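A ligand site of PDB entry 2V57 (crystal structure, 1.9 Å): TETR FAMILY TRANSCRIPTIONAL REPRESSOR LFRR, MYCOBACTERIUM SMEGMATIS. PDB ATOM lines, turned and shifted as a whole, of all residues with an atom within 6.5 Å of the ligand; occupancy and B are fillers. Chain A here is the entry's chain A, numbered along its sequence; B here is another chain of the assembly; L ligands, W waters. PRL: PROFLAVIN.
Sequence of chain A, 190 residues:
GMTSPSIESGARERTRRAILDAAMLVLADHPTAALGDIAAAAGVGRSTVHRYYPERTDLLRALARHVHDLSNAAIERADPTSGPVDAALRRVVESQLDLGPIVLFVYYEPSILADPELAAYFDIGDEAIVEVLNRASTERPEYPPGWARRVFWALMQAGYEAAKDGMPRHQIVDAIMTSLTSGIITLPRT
OG of Ser 71 sits at hydrogen-bond distance from N15 of the ligand.
A nitrogen (N10) of the ligand lies within hydrogen-bond range of the side-chain hydroxyl of Tyr 107 (3.0 Å).
OD1 of Asn 72 lies within hydrogen-bond range of N15 of the ligand (3.0 Å).
Residues that only touch the ligand: His 68 (3.3 Å), Asp 126 (3.3 Å), Trp 153 (3.4 Å), Arg 149 (3.4 Å), Ile 75 (3.6 Å), Phe 122 (3.7 Å), Ile 124 (3.9 Å) and Gly 125 (3.99 Å).
Hydrophobic or aromatic side chains within 4 Å of the ligand: His 68, Ile 75, Tyr 107 and Trp 153.
OD2 of Asp 126 lies within hydrogen-bond range of NE1 of Trp 153, 2.9 Å away.
A ring nitrogen (NE2) of His 68 is in hydrogen-bond range of the backbone carbonyl oxygen of Ile 124.
OD2 of Asp 126 is in salt-bridge range of NE of Arg 149 (2.8 Å).
A ring nitrogen (NE2) of His 68 sits close to the backbone carbonyl oxygen (O) of Phe 122.
The guanidinium group of Arg 149 is in salt-bridge range of the side-chain carboxylate of Asp 123.
A ring nitrogen (NE2) of His 68 sits at hydrogen-bond distance from the side-chain amide nitrogen of Asn 72, 3.4 Å away.
The backbone NH (N) of Gly 125 sits at hydrogen-bond distance from the side-chain carboxylate (OE2) of Glu 127, 3.1 Å away.
OE1 of Gln 96 is in hydrogen-bond range of OG of Ser 71 (2.6 Å).
Water W2 lies within hydrogen-bond range of OH of Tyr 107 (2.7 Å) and O of Phe 122 (2.9 Å).
Water W1 lies within hydrogen-bond range of the backbone carbonyl oxygen (O) of Arg 150 (2.7 Å) and a nitrogen (N16) of the ligand (3.4 Å).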
ATOM      1  N   VAL A  67      15.405 -15.208 -19.076  1.00  0.00           N
ATOM      2  CA  VAL A  67      14.286 -15.748 -18.296  1.00  0.00           C
ATOM      3  C   VAL A  67      14.702 -17.002 -17.516  1.00  0.00           C
ATOM      4  O   VAL A  67      14.352 -17.160 -16.334  1.00  0.00           O
ATOM      5  CB  VAL A  67      13.057 -16.054 -19.197  1.00  0.00           C
ATOM      6  CG1 VAL A  67      12.045 -16.900 -18.424  1.00  0.00           C
ATOM      7  CG2 VAL A  67      12.403 -14.732 -19.650  1.00  0.00           C
ATOM      8  N   HIS A  68      15.462 -17.865 -18.173  1.00  0.00           N
ATOM      9  CA  HIS A  68      15.941 -19.064 -17.519  1.00  0.00           C
ATOM     10  C   HIS A  68      16.881 -18.703 -16.358  1.00  0.00           C
ATOM     11  O   HIS A  68      16.802 -19.296 -15.274  1.00  0.00           O
ATOM     12  CB  HIS A  68      16.616 -20.014 -18.517  1.00  0.00           C
ATOM     13  CG  HIS A  68      16.947 -21.354 -17.928  1.00  0.00           C
ATOM     14  ND1 HIS A  68      15.980 -22.273 -17.560  1.00  0.00           N
ATOM     15  CD2 HIS A  68      18.136 -21.931 -17.634  1.00  0.00           C
ATOM     16  CE1 HIS A  68      16.554 -23.347 -17.066  1.00  0.00           C
ATOM     17  NE2 HIS A  68      17.862 -23.174 -17.090  1.00  0.00           N
ATOM     18  N   SER A  71      14.819 -17.588 -13.546  1.00  0.00           N
ATOM     19  CA  SER A  71      14.167 -18.754 -12.973  1.00  0.00           C
ATOM     20  C   SER A  71      15.138 -19.474 -12.031  1.00  0.00           C
ATOM     21  O   SER A  71      14.779 -19.837 -10.903  1.00  0.00           O
ATOM     22  CB  SER A  71      13.666 -19.696 -14.075  1.00  0.00           C
ATOM     23  OG  SER A  71      13.139 -20.908 -13.543  1.00  0.00           O
ATOM     24  N   ASN A  72      16.356 -19.704 -12.504  1.00  0.00           N
ATOM     25  CA  ASN A  72      17.398 -20.312 -11.647  1.00  0.00           C
ATOM     26  C   ASN A  72      17.721 -19.503 -10.390  1.00  0.00           C
ATOM     27  O   ASN A  72      17.987 -20.070  -9.322  1.00  0.00           O
ATOM     28  CB  ASN A  72      18.671 -20.586 -12.448  1.00  0.00           C
ATOM     29  CG  ASN A  72      18.557 -21.846 -13.333  1.00  0.00           C
ATOM     30  OD1 ASN A  72      17.742 -22.742 -13.059  1.00  0.00           O
ATOM     31  ND2 ASN A  72      19.362 -21.898 -14.371  1.00  0.00           N
ATOM     32  N   ILE A  75      14.998 -20.087  -7.923  1.00  0.00           N
ATOM     33  CA  ILE A  75      15.139 -21.387  -7.262  1.00  0.00           C
ATOM     34  C   ILE A  75      16.172 -21.315  -6.138  1.00  0.00           C
ATOM     35  O   ILE A  75      15.918 -21.773  -5.004  1.00  0.00           O
ATOM     36  CB  ILE A  75      15.512 -22.498  -8.263  1.00  0.00           C
ATOM     37  CG1 ILE A  75      14.363 -22.668  -9.278  1.00  0.00           C
ATOM     38  CG2 ILE A  75      15.855 -23.802  -7.493  1.00  0.00           C
ATOM     39  CD1 ILE A  75      14.710 -23.599 -10.465  1.00  0.00           C
ATOM     40  N   GLN A  96       8.503 -18.962  -8.824  1.00  0.00           N
ATOM     41  CA  GLN A  96       8.423 -19.299 -10.257  1.00  0.00           C
ATOM     42  C   GLN A  96       7.189 -18.601 -10.858  1.00  0.00           C
ATOM     43  O   GLN A  96       7.252 -18.022 -11.945  1.00  0.00           O
ATOM     44  CB  GLN A  96       8.378 -20.833 -10.515  1.00  0.00           C
ATOM     45  CG  GLN A  96       9.689 -21.613 -10.178  1.00  0.00           C
ATOM     46  CD  GLN A  96      10.900 -21.036 -10.908  1.00  0.00           C
ATOM     47  OE1 GLN A  96      10.927 -20.987 -12.128  1.00  0.00           O
ATOM     48  NE2 GLN A  96      11.900 -20.601 -10.141  1.00  0.00           N
ATOM     49  N   TYR A 107       8.867 -21.174 -23.766  1.00  0.00           N
ATOM     50  CA  TYR A 107       8.796 -22.595 -24.038  1.00  0.00           C
ATOM     51  C   TYR A 107       8.017 -22.951 -25.303  1.00  0.00           C
ATOM     52  O   TYR A 107       8.256 -23.988 -25.904  1.00  0.00           O
ATOM     53  CB  TYR A 107       8.235 -23.347 -22.816  1.00  0.00           C
ATOM     54  CG  TYR A 107       9.286 -23.549 -21.763  1.00  0.00           C
ATOM     55  CD1 TYR A 107      10.068 -24.706 -21.743  1.00  0.00           C
ATOM     56  CD2 TYR A 107       9.520 -22.579 -20.796  1.00  0.00           C
ATOM     57  CE1 TYR A 107      11.063 -24.882 -20.784  1.00  0.00           C
ATOM     58  CE2 TYR A 107      10.518 -22.753 -19.828  1.00  0.00           C
ATOM     59  CZ  TYR A 107      11.274 -23.905 -19.822  1.00  0.00           C
ATOM     60  OH  TYR A 107      12.243 -24.065 -18.858  1.00  0.00           O
ATOM     61  N   TYR A 121      21.232 -25.651 -22.177  1.00  0.00           N
ATOM     62  CA  TYR A 121      21.251 -24.682 -21.090  1.00  0.00           C
ATOM     63  C   TYR A 121      19.965 -24.716 -20.280  1.00  0.00           C
ATOM     64  O   TYR A 121      19.979 -24.621 -19.057  1.00  0.00           O
ATOM     65  CB  TYR A 121      21.431 -23.278 -21.668  1.00  0.00           C
ATOM     66  CG  TYR A 121      21.798 -22.204 -20.677  1.00  0.00           C
ATOM     67  CD1 TYR A 121      23.067 -22.172 -20.098  1.00  0.00           C
ATOM     68  CD2 TYR A 121      20.894 -21.214 -20.340  1.00  0.00           C
ATOM     69  CE1 TYR A 121      23.408 -21.195 -19.198  1.00  0.00           C
ATOM     70  CE2 TYR A 121      21.231 -20.227 -19.430  1.00  0.00           C
ATOM     71  CZ  TYR A 121      22.487 -20.219 -18.863  1.00  0.00           C
ATOM     72  OH  TYR A 121      22.815 -19.238 -17.981  1.00  0.00           O
ATOM     73  N   PHE A 122      18.841 -24.866 -20.967  1.00  0.00           N
ATOM     74  CA  PHE A 122      17.535 -24.892 -20.301  1.00  0.00           C
ATOM     75  C   PHE A 122      17.345 -26.104 -19.405  1.00  0.00           C
ATOM     76  O   PHE A 122      16.541 -26.081 -18.479  1.00  0.00           O
ATOM     77  CB  PHE A 122      16.392 -24.800 -21.337  1.00  0.00           C
ATOM     78  CG  PHE A 122      15.834 -23.419 -21.479  1.00  0.00           C
ATOM     79  CD1 PHE A 122      14.521 -23.153 -21.164  1.00  0.00           C
ATOM     80  CD2 PHE A 122      16.645 -22.379 -21.907  1.00  0.00           C
ATOM     81  CE1 PHE A 122      14.007 -21.870 -21.281  1.00  0.00           C
ATOM     82  CE2 PHE A 122      16.138 -21.103 -22.024  1.00  0.00           C
ATOM     83  CZ  PHE A 122      14.821 -20.853 -21.716  1.00  0.00           C
ATOM     84  N   ASP A 123      18.095 -27.171 -19.669  1.00  0.00           N
ATOM     85  CA  ASP A 123      17.950 -28.388 -18.871  1.00  0.00           C
ATOM     86  C   ASP A 123      18.621 -28.284 -17.503  1.00  0.00           C
ATOM     87  O   ASP A 123      18.423 -29.151 -16.649  1.00  0.00           O
ATOM     88  CB  ASP A 123      18.484 -29.605 -19.625  1.00  0.00           C
ATOM     89  CG  ASP A 123      17.923 -30.902 -19.087  1.00  0.00           C
ATOM     90  OD1 ASP A 123      16.713 -30.961 -18.764  1.00  0.00           O
ATOM     91  OD2 ASP A 123      18.687 -31.879 -19.001  1.00  0.00           O
ATOM     92  N   ILE A 124      19.365 -27.200 -17.270  1.00  0.00           N
ATOM     93  CA  ILE A 124      20.177 -27.050 -16.061  1.00  0.00           C
ATOM     94  C   ILE A 124      19.606 -26.036 -15.054  1.00  0.00           C
ATOM     95  O   ILE A 124      19.319 -24.894 -15.395  1.00  0.00           O
ATOM     96  CB  ILE A 124      21.598 -26.611 -16.446  1.00  0.00           C
ATOM     97  CG1 ILE A 124      22.238 -27.653 -17.362  1.00  0.00           C
ATOM     98  CG2 ILE A 124      22.467 -26.373 -15.219  1.00  0.00           C
ATOM     99  CD1 ILE A 124      23.418 -27.110 -18.162  1.00  0.00           C
ATOM    100  N   GLY A 125      19.457 -26.451 -13.801  1.00  0.00           N
ATOM    101  CA  GLY A 125      19.167 -25.484 -12.756  1.00  0.00           C
ATOM    102  C   GLY A 125      18.228 -25.931 -11.667  1.00  0.00           C
ATOM    103  O   GLY A 125      18.224 -25.330 -10.588  1.00  0.00           O
ATOM    104  N   ASP A 126      17.440 -26.971 -11.938  1.00  0.00           N
ATOM    105  CA  ASP A 126      16.369 -27.347 -11.012  1.00  0.00           C
ATOM    106  C   ASP A 126      16.730 -28.560 -10.181  1.00  0.00           C
ATOM    107  O   ASP A 126      15.848 -29.242  -9.660  1.00  0.00           O
ATOM    108  CB  ASP A 126      15.034 -27.599 -11.763  1.00  0.00           C
ATOM    109  CG  ASP A 126      15.068 -28.831 -12.678  1.00  0.00           C
ATOM    110  OD1 ASP A 126      16.174 -29.261 -13.078  1.00  0.00           O
ATOM    111  OD2 ASP A 126      13.980 -29.356 -12.996  1.00  0.00           O
ATOM    112  N   GLU A 127      18.029 -28.824 -10.044  1.00  0.00           N
ATOM    113  CA  GLU A 127      18.449 -30.061  -9.407  1.00  0.00           C
ATOM    114  C   GLU A 127      17.983 -30.158  -7.957  1.00  0.00           C
ATOM    115  O   GLU A 127      17.677 -31.238  -7.465  1.00  0.00           O
ATOM    116  CB  GLU A 127      19.960 -30.276  -9.516  1.00  0.00           C
ATOM    117  CG  GLU A 127      20.433 -30.415 -10.956  1.00  0.00           C
ATOM    118  CD  GLU A 127      20.549 -29.069 -11.685  1.00  0.00           C
ATOM    119  OE1 GLU A 127      20.316 -28.017 -11.046  1.00  0.00           O
ATOM    120  OE2 GLU A 127      20.872 -29.066 -12.892  1.00  0.00           O
ATOM    121  N   ILE A 129      15.218 -28.888  -6.733  1.00  0.00           N
ATOM    122  CA  ILE A 129      13.776 -29.156  -6.692  1.00  0.00           C
ATOM    123  C   ILE A 129      13.599 -30.654  -6.853  1.00  0.00           C
ATOM    124  O   ILE A 129      12.818 -31.304  -6.125  1.00  0.00           O
ATOM    125  CB  ILE A 129      12.996 -28.413  -7.794  1.00  0.00           C
ATOM    126  CG1 ILE A 129      13.165 -26.892  -7.667  1.00  0.00           C
ATOM    127  CG2 ILE A 129      11.506 -28.829  -7.774  1.00  0.00           C
ATOM    128  CD1 ILE A 129      12.466 -26.117  -8.779  1.00  0.00           C
ATOM    129  N   ARG A 149       9.900 -34.969 -12.121  1.00  0.00           N
ATOM    130  CA  ARG A 149      10.350 -33.644 -12.565  1.00  0.00           C
ATOM    131  C   ARG A 149       9.431 -33.093 -13.662  1.00  0.00           C
ATOM    132  O   ARG A 149       9.034 -31.920 -13.634  1.00  0.00           O
ATOM    133  CB  ARG A 149      11.785 -33.744 -13.087  1.00  0.00           C
ATOM    134  CG  ARG A 149      12.303 -32.464 -13.715  1.00  0.00           C
ATOM    135  CD  ARG A 149      13.623 -32.755 -14.453  1.00  0.00           C
ATOM    136  NE  ARG A 149      14.420 -31.546 -14.643  1.00  0.00           N
ATOM    137  CZ  ARG A 149      15.266 -31.377 -15.650  1.00  0.00           C
ATOM    138  NH1 ARG A 149      15.387 -32.316 -16.574  1.00  0.00           N
ATOM    139  NH2 ARG A 149      15.988 -30.256 -15.747  1.00  0.00           N
ATOM    140  N   ARG A 150       9.064 -33.928 -14.613  1.00  0.00           N
ATOM    141  CA  ARG A 150       8.142 -33.504 -15.663  1.00  0.00           C
ATOM    142  C   ARG A 150       6.792 -33.090 -15.110  1.00  0.00           C
ATOM    143  O   ARG A 150       6.181 -32.155 -15.619  1.00  0.00           O
ATOM    144  CB  ARG A 150       7.918 -34.638 -16.655  1.00  0.00           C
ATOM    145  CG  ARG A 150       9.167 -35.102 -17.359  1.00  0.00           C
ATOM    146  CD  ARG A 150       8.808 -36.033 -18.507  1.00  0.00           C
ATOM    147  NE  ARG A 150       9.991 -36.646 -19.099  1.00  0.00           N
ATOM    148  CZ  ARG A 150      10.777 -36.083 -20.013  1.00  0.00           C
ATOM    149  NH1 ARG A 150      10.538 -34.862 -20.459  1.00  0.00           N
ATOM    150  NH2 ARG A 150      11.814 -36.756 -20.484  1.00  0.00           N
ATOM    151  N   TRP A 153       6.860 -29.487 -13.411  1.00  0.00           N
ATOM    152  CA  TRP A 153       6.844 -28.373 -14.352  1.00  0.00           C
ATOM    153  C   TRP A 153       5.565 -28.340 -15.185  1.00  0.00           C
ATOM    154  O   TRP A 153       5.154 -27.282 -15.674  1.00  0.00           O
ATOM    155  CB  TRP A 153       8.094 -28.364 -15.253  1.00  0.00           C
ATOM    156  CG  TRP A 153       9.349 -28.039 -14.469  1.00  0.00           C
ATOM    157  CD1 TRP A 153      10.383 -28.885 -14.204  1.00  0.00           C
ATOM    158  CD2 TRP A 153       9.664 -26.808 -13.822  1.00  0.00           C
ATOM    159  NE1 TRP A 153      11.331 -28.255 -13.437  1.00  0.00           N
ATOM    160  CE2 TRP A 153      10.915 -26.969 -13.201  1.00  0.00           C
ATOM    161  CE3 TRP A 153       9.020 -25.566 -13.720  1.00  0.00           C
ATOM    162  CZ2 TRP A 153      11.535 -25.944 -12.471  1.00  0.00           C
ATOM    163  CZ3 TRP A 153       9.637 -24.553 -13.019  1.00  0.00           C
ATOM    164  CH2 TRP A 153      10.885 -24.744 -12.401  1.00  0.00           C
ATOM    165  N   ALA A 154       4.917 -29.495 -15.328  1.00  0.00           N
ATOM    166  CA  ALA A 154       3.597 -29.556 -15.950  1.00  0.00           C
ATOM    167  C   ALA A 154       2.560 -28.823 -15.097  1.00  0.00           C
ATOM    168  O   ALA A 154       1.726 -28.072 -15.609  1.00  0.00           O
ATOM    169  CB  ALA A 154       3.165 -30.994 -16.192  1.00  0.00           C
ATOM    170  N   GLN A 157       3.177 -25.198 -15.445  1.00  0.00           N
ATOM    171  CA  GLN A 157       2.548 -24.738 -16.689  1.00  0.00           C
ATOM    172  C   GLN A 157       1.066 -24.432 -16.554  1.00  0.00           C
ATOM    173  O   GLN A 157       0.594 -23.377 -17.023  1.00  0.00           O
ATOM    174  CB  GLN A 157       2.735 -25.749 -17.822  1.00  0.00           C
ATOM    175  CG  GLN A 157       2.081 -25.242 -19.088  1.00  0.00           C
ATOM    176  CD  GLN A 157       2.135 -26.223 -20.227  1.00  0.00           C
ATOM    177  OE1 GLN A 157       1.099 -26.688 -20.711  1.00  0.00           O
ATOM    178  NE2 GLN A 157       3.330 -26.531 -20.656  1.00  0.00           N
ATOM    179  N   GLU B 161       6.751 -35.362 -24.509  1.00  0.00           N
ATOM    180  CA  GLU B 161       8.175 -35.107 -24.287  1.00  0.00           C
ATOM    181  C   GLU B 161       8.882 -36.389 -23.890  1.00  0.00           C
ATOM    182  O   GLU B 161       9.964 -36.697 -24.401  1.00  0.00           O
ATOM    183  CB  GLU B 161       8.387 -34.060 -23.189  1.00  0.00           C
ATOM    184  CG  GLU B 161       7.621 -32.766 -23.389  1.00  0.00           C
ATOM    185  CD  GLU B 161       8.409 -31.731 -24.139  1.00  0.00           C
ATOM    186  OE1 GLU B 161       9.115 -32.106 -25.106  1.00  0.00           O
ATOM    187  OE2 GLU B 161       8.326 -30.537 -23.755  1.00  0.00           O
HETATM  188  C1  PRL L   1      15.173 -26.543 -15.114  1.00  0.00           C
HETATM  189  C2  PRL L   1      15.503 -25.321 -14.513  1.00  0.00           C
HETATM  190  C3  PRL L   1      14.594 -24.261 -14.560  1.00  0.00           C
HETATM  191  C4  PRL L   1      13.363 -24.418 -15.180  1.00  0.00           C
HETATM  192  C5  PRL L   1      10.219 -26.993 -17.620  1.00  0.00           C
HETATM  193  C6  PRL L   1       9.833 -28.181 -18.243  1.00  0.00           C
HETATM  194  C7  PRL L   1      10.687 -29.274 -18.225  1.00  0.00           C
HETATM  195  C8  PRL L   1      11.927 -29.176 -17.608  1.00  0.00           C
HETATM  196  C9  PRL L   1      13.573 -27.898 -16.372  1.00  0.00           C
HETATM  197  N10 PRL L   1      11.836 -25.753 -16.400  1.00  0.00           N
HETATM  198  C11 PRL L   1      13.040 -25.619 -15.788  1.00  0.00           C
HETATM  199  C12 PRL L   1      12.316 -27.997 -16.995  1.00  0.00           C
HETATM  200  C13 PRL L   1      13.929 -26.695 -15.753  1.00  0.00           C
HETATM  201  C14 PRL L   1      11.462 -26.907 -16.990  1.00  0.00           C
HETATM  202  N15 PRL L   1      14.908 -23.079 -13.977  1.00  0.00           N
HETATM  203  N16 PRL L   1       8.626 -28.292 -18.847  1.00  0.00           N
HETATM  204  O   HOH W   1       6.811 -31.010 -18.033  1.00  0.00           O
HETATM  205  O   HOH W   2      13.815 -26.263 -19.301  1.00  0.00           O
